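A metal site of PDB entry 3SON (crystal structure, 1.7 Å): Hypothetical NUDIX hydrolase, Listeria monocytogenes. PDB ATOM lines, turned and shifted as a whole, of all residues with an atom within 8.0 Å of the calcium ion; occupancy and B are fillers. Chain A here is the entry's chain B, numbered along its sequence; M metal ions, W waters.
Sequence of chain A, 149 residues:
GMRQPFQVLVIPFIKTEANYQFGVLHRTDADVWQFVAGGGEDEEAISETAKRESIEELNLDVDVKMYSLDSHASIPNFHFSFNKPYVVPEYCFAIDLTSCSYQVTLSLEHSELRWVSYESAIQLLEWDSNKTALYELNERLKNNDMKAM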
ATOM      1  N   GLN A   7      33.198   0.065 -16.689  1.00  0.00           N
ATOM      2  CA  GLN A   7      32.368   0.712 -15.663  1.00  0.00           C
ATOM      3  C   GLN A   7      31.034   0.019 -15.655  1.00  0.00           C
ATOM      4  O   GLN A   7      30.669  -0.582 -16.650  1.00  0.00           O
ATOM      5  CB  GLN A   7      32.082   2.184 -16.008  1.00  0.00           C
ATOM      6  CG  GLN A   7      33.250   3.104 -15.922  1.00  0.00           C
ATOM      7  CD  GLN A   7      33.609   3.468 -14.453  1.00  0.00           C
ATOM      8  OE1 GLN A   7      32.764   3.934 -13.662  1.00  0.00           O
ATOM      9  NE2 GLN A   7      34.809   3.215 -14.096  1.00  0.00           N
ATOM     10  N   VAL A   8      30.309   0.144 -14.555  1.00  0.00           N
ATOM     11  CA  VAL A   8      28.970  -0.385 -14.444  1.00  0.00           C
ATOM     12  C   VAL A   8      28.031   0.750 -14.025  1.00  0.00           C
ATOM     13  O   VAL A   8      28.494   1.746 -13.422  1.00  0.00           O
ATOM     14  CB  VAL A   8      28.864  -1.578 -13.453  1.00  0.00           C
ATOM     15  CG1 VAL A   8      29.778  -2.784 -13.843  1.00  0.00           C
ATOM     16  CG2 VAL A   8      29.110  -1.128 -12.046  1.00  0.00           C
ATOM     17  N   LEU A  25      19.995   9.388  -7.715  1.00  0.00           N
ATOM     18  CA  LEU A  25      20.955   9.870  -6.721  1.00  0.00           C
ATOM     19  C   LEU A  25      21.495  11.243  -7.088  1.00  0.00           C
ATOM     20  O   LEU A  25      21.881  11.478  -8.244  1.00  0.00           O
ATOM     21  CB  LEU A  25      22.067   8.864  -6.501  1.00  0.00           C
ATOM     22  CG  LEU A  25      21.732   7.376  -6.426  1.00  0.00           C
ATOM     23  CD1 LEU A  25      23.032   6.518  -6.441  1.00  0.00           C
ATOM     24  CD2 LEU A  25      20.773   7.022  -5.330  1.00  0.00           C
ATOM     25  N   ARG A  27      24.450  14.072  -6.565  1.00  0.00           N
ATOM     26  CA  ARG A  27      25.800  14.311  -6.100  1.00  0.00           C
ATOM     27  C   ARG A  27      25.858  15.530  -5.184  1.00  0.00           C
ATOM     28  O   ARG A  27      24.957  16.342  -5.158  1.00  0.00           O
ATOM     29  CB  ARG A  27      26.700  14.561  -7.275  1.00  0.00           C
ATOM     30  CG  ARG A  27      26.813  13.408  -8.244  1.00  0.00           C
ATOM     31  CD  ARG A  27      27.827  13.740  -9.326  1.00  0.00           C
ATOM     32  NE  ARG A  27      29.192  13.714  -8.800  1.00  0.00           N
ATOM     33  CZ  ARG A  27      30.033  12.690  -8.878  1.00  0.00           C
ATOM     34  NH1 ARG A  27      29.671  11.530  -9.420  1.00  0.00           N
ATOM     35  NH2 ARG A  27      31.250  12.829  -8.354  1.00  0.00           N
ATOM     36  N   GLN A  34      22.110  11.006 -11.022  1.00  0.00           N
ATOM     37  CA  GLN A  34      22.658   9.884 -11.697  1.00  0.00           C
ATOM     38  C   GLN A  34      22.207   8.591 -11.006  1.00  0.00           C
ATOM     39  O   GLN A  34      21.454   8.600 -10.053  1.00  0.00           O
ATOM     40  CB  GLN A  34      24.220   9.938 -11.593  1.00  0.00           C
ATOM     41  CG  GLN A  34      24.757   9.975 -10.172  1.00  0.00           C
ATOM     42  CD  GLN A  34      26.289  10.051 -10.030  1.00  0.00           C
ATOM     43  OE1 GLN A  34      26.891  11.062 -10.332  1.00  0.00           O
ATOM     44  NE2 GLN A  34      26.907   8.984  -9.512  1.00  0.00           N
ATOM     45  N   PHE A  35      22.696   7.466 -11.518  1.00  0.00           N
ATOM     46  CA  PHE A  35      22.430   6.211 -10.860  1.00  0.00           C
ATOM     47  C   PHE A  35      23.669   5.665 -10.179  1.00  0.00           C
ATOM     48  O   PHE A  35      24.672   6.367  -9.999  1.00  0.00           O
ATOM     49  CB  PHE A  35      21.849   5.185 -11.840  1.00  0.00           C
ATOM     50  CG  PHE A  35      20.488   5.563 -12.377  1.00  0.00           C
ATOM     51  CD1 PHE A  35      19.384   5.705 -11.529  1.00  0.00           C
ATOM     52  CD2 PHE A  35      20.297   5.714 -13.760  1.00  0.00           C
ATOM     53  CE1 PHE A  35      18.116   6.004 -12.052  1.00  0.00           C
ATOM     54  CE2 PHE A  35      19.044   5.998 -14.292  1.00  0.00           C
ATOM     55  CZ  PHE A  35      17.941   6.139 -13.443  1.00  0.00           C
ATOM     56  N   VAL A  36      23.574   4.438  -9.683  1.00  0.00           N
ATOM     57  CA  VAL A  36      24.726   3.808  -9.063  1.00  0.00           C
ATOM     58  C   VAL A  36      25.755   3.552 -10.173  1.00  0.00           C
ATOM     59  O   VAL A  36      25.417   3.028 -11.184  1.00  0.00           O
ATOM     60  CB  VAL A  36      24.335   2.468  -8.395  1.00  0.00           C
ATOM     61  CG1 VAL A  36      25.584   1.623  -7.957  1.00  0.00           C
ATOM     62  CG2 VAL A  36      23.325   2.704  -7.261  1.00  0.00           C
ATOM     63  N   ALA A  37      27.016   3.867  -9.918  1.00  0.00           N
ATOM     64  CA  ALA A  37      28.090   3.716 -10.878  1.00  0.00           C
ATOM     65  C   ALA A  37      29.445   3.437 -10.253  1.00  0.00           C
ATOM     66  O   ALA A  37      29.781   3.921  -9.122  1.00  0.00           O
ATOM     67  CB  ALA A  37      28.197   4.969 -11.756  1.00  0.00           C
ATOM     68  N   GLY A  38      30.296   2.684 -10.948  1.00  0.00           N
ATOM     69  CA  GLY A  38      31.664   2.478 -10.454  1.00  0.00           C
ATOM     70  C   GLY A  38      32.474   1.597 -11.391  1.00  0.00           C
ATOM     71  O   GLY A  38      31.911   1.046 -12.314  1.00  0.00           O
ATOM     72  N   GLY A  39      33.772   1.469 -11.132  1.00  0.00           N
ATOM     73  CA  GLY A  39      34.703   0.695 -11.988  1.00  0.00           C
ATOM     74  C   GLY A  39      34.956  -0.730 -11.513  1.00  0.00           C
ATOM     75  O   GLY A  39      34.820  -1.050 -10.321  1.00  0.00           O
ATOM     76  N   GLU A  41      37.070  -3.704 -10.356  1.00  0.00           N
ATOM     77  CA  GLU A  41      38.251  -3.821  -9.504  1.00  0.00           C
ATOM     78  C   GLU A  41      38.850  -5.185  -9.652  1.00  0.00           C
ATOM     79  O   GLU A  41      38.137  -6.150  -9.880  1.00  0.00           O
ATOM     80  CB  GLU A  41      37.872  -3.552  -8.038  1.00  0.00           C
ATOM     81  CG  GLU A  41      37.659  -2.082  -7.769  1.00  0.00           C
ATOM     82  CD  GLU A  41      37.094  -1.770  -6.370  1.00  0.00           C
ATOM     83  OE1 GLU A  41      36.859  -2.715  -5.572  1.00  0.00           O
ATOM     84  OE2 GLU A  41      36.848  -0.558  -6.077  1.00  0.00           O
ATOM     85  N   ARG A  52      28.449  -5.332  -6.079  1.00  0.00           N
ATOM     86  CA  ARG A  52      29.247  -4.754  -5.054  1.00  0.00           C
ATOM     87  C   ARG A  52      28.921  -3.300  -4.917  1.00  0.00           C
ATOM     88  O   ARG A  52      28.718  -2.810  -3.814  1.00  0.00           O
ATOM     89  CB  ARG A  52      30.767  -4.910  -5.311  1.00  0.00           C
ATOM     90  CG  ARG A  52      31.574  -4.358  -4.180  1.00  0.00           C
ATOM     91  CD  ARG A  52      33.107  -4.349  -4.359  1.00  0.00           C
ATOM     92  NE  ARG A  52      33.586  -4.031  -5.712  1.00  0.00           N
ATOM     93  CZ  ARG A  52      33.530  -2.851  -6.306  1.00  0.00           C
ATOM     94  NH1 ARG A  52      33.148  -1.736  -5.650  1.00  0.00           N
ATOM     95  NH2 ARG A  52      34.026  -2.746  -7.520  1.00  0.00           N
ATOM     96  N   GLU A  53      28.970  -2.591  -6.034  1.00  0.00           N
ATOM     97  CA  GLU A  53      28.770  -1.122  -6.000  1.00  0.00           C
ATOM     98  C   GLU A  53      27.344  -0.829  -5.448  1.00  0.00           C
ATOM     99  O   GLU A  53      27.163   0.086  -4.627  1.00  0.00           O
ATOM    100  CB  GLU A  53      28.961  -0.506  -7.384  1.00  0.00           C
ATOM    101  CG  GLU A  53      30.392  -0.521  -7.943  1.00  0.00           C
ATOM    102  CD  GLU A  53      31.311   0.570  -7.361  1.00  0.00           C
ATOM    103  OE1 GLU A  53      30.763   1.634  -6.972  1.00  0.00           O
ATOM    104  OE2 GLU A  53      32.533   0.387  -7.414  1.00  0.00           O
ATOM    105  N   SER A  54      26.402  -1.704  -5.802  1.00  0.00           N
ATOM    106  CA  SER A  54      24.987  -1.576  -5.329  1.00  0.00           C
ATOM    107  C   SER A  54      24.927  -1.701  -3.812  1.00  0.00           C
ATOM    108  O   SER A  54      24.329  -0.872  -3.128  1.00  0.00           O
ATOM    109  CB  SER A  54      24.089  -2.648  -5.954  1.00  0.00           C
ATOM    110  OG  SER A  54      24.003  -2.426  -7.347  1.00  0.00           O
ATOM    111  N   GLU A  56      27.332  -1.473  -1.578  1.00  0.00           N
ATOM    112  CA  GLU A  56      28.040  -0.416  -0.937  1.00  0.00           C
ATOM    113  C   GLU A  56      27.366   0.958  -0.976  1.00  0.00           C
ATOM    114  O   GLU A  56      27.340   1.652   0.054  1.00  0.00           O
ATOM    115  CB  GLU A  56      29.393  -0.273  -1.573  1.00  0.00           C
ATOM    116  CG  GLU A  56      30.228  -1.523  -1.316  1.00  0.00           C
ATOM    117  CD  GLU A  56      31.599  -1.428  -1.892  1.00  0.00           C
ATOM    118  OE1 GLU A  56      31.881  -0.372  -2.526  1.00  0.00           O
ATOM    119  OE2 GLU A  56      32.387  -2.403  -1.683  1.00  0.00           O
ATOM    120  N   GLU A  57      26.913   1.374  -2.149  1.00  0.00           N
ATOM    121  CA  GLU A  57      26.362   2.695  -2.298  1.00  0.00           C
ATOM    122  C   GLU A  57      25.045   2.802  -1.556  1.00  0.00           C
ATOM    123  O   GLU A  57      24.682   3.892  -1.062  1.00  0.00           O
ATOM    124  CB  GLU A  57      26.212   3.078  -3.762  1.00  0.00           C
ATOM    125  CG  GLU A  57      27.523   3.237  -4.551  1.00  0.00           C
ATOM    126  CD  GLU A  57      27.301   4.077  -5.810  1.00  0.00           C
ATOM    127  OE1 GLU A  57      26.302   4.829  -5.833  1.00  0.00           O
ATOM    128  OE2 GLU A  57      28.103   3.965  -6.782  1.00  0.00           O
ATOM    129  N   SER A 107      28.392  10.670   0.514  1.00  0.00           N
ATOM    130  CA  SER A 107      29.645  10.939  -0.181  1.00  0.00           C
ATOM    131  C   SER A 107      29.478  12.009  -1.256  1.00  0.00           C
ATOM    132  O   SER A 107      28.369  12.501  -1.577  1.00  0.00           O
ATOM    133  CB  SER A 107      30.272   9.650  -0.759  1.00  0.00           C
ATOM    134  OG  SER A 107      29.693   9.224  -1.985  1.00  0.00           O
ATOM    135  N   GLU A 109      29.901  11.645  -4.352  1.00  0.00           N
ATOM    136  CA  GLU A 109      29.125  11.039  -5.452  1.00  0.00           C
ATOM    137  C   GLU A 109      27.590  11.056  -5.246  1.00  0.00           C
ATOM    138  O   GLU A 109      26.827  10.985  -6.201  1.00  0.00           O
ATOM    139  CB  GLU A 109      29.565   9.591  -5.657  1.00  0.00           C
ATOM    140  CG  GLU A 109      31.048   9.400  -5.957  1.00  0.00           C
ATOM    141  CD  GLU A 109      31.411   7.933  -6.193  1.00  0.00           C
ATOM    142  OE1 GLU A 109      30.607   7.028  -5.862  1.00  0.00           O
ATOM    143  OE2 GLU A 109      32.520   7.681  -6.707  1.00  0.00           O
ATOM    144  N   HIS A 110      27.132  11.101  -4.005  1.00  0.00           N
ATOM    145  CA  HIS A 110      25.715  11.111  -3.703  1.00  0.00           C
ATOM    146  C   HIS A 110      25.406  11.357  -2.240  1.00  0.00           C
ATOM    147  O   HIS A 110      25.926  10.657  -1.363  1.00  0.00           O
ATOM    148  CB  HIS A 110      25.067   9.802  -4.111  1.00  0.00           C
ATOM    149  CG  HIS A 110      25.916   8.625  -3.874  1.00  0.00           C
ATOM    150  ND1 HIS A 110      26.358   8.293  -2.631  1.00  0.00           N
ATOM    151  CD2 HIS A 110      26.477   7.729  -4.751  1.00  0.00           C
ATOM    152  CE1 HIS A 110      27.145   7.216  -2.719  1.00  0.00           C
ATOM    153  NE2 HIS A 110      27.210   6.861  -4.024  1.00  0.00           N
HETATM  154 CA    CA M   1      30.638   4.282  -6.963  1.00  0.00          CA
HETATM  155  O   HOH W   1      33.249   4.088  -7.590  1.00  0.00           O
HETATM  156  O   HOH W   2      29.131   6.679  -8.163  1.00  0.00           O
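The side-chain carboxylate (OE1) of Glu 57 is in hydrogen-bond range of a ring nitrogen (NE2) of His 110 (2.9 Å).
The guanidinium group of Arg 52 lies within salt-bridge range of the side-chain carboxylate of Glu 53 (2.8 Å).
The backbone NH (N) of Glu 109 sits close to the side-chain hydroxyl (OG) of Ser 107 (3.4 Å).
Four residues have an atom within 4 Å of the calcium ion: Ala 37, Glu 53, Glu 57 and Glu 109.
The calcium ion is bound by O of Ala 37 (2.4 Å), OE2 of Glu 57 (2.6 Å), OE1 of Glu 53 (2.7 Å) and water W1 (2.7 Å).
Slightly farther from the calcium ion lies OE1 of Glu 109 (3.0 Å).
Slightly farther from the calcium ion lies water W2 (3.1 Å).
Water W2 bridges OE1 of Glu 109 (2.8 Å) and NE2 of Gln 34 (3.5 Å).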
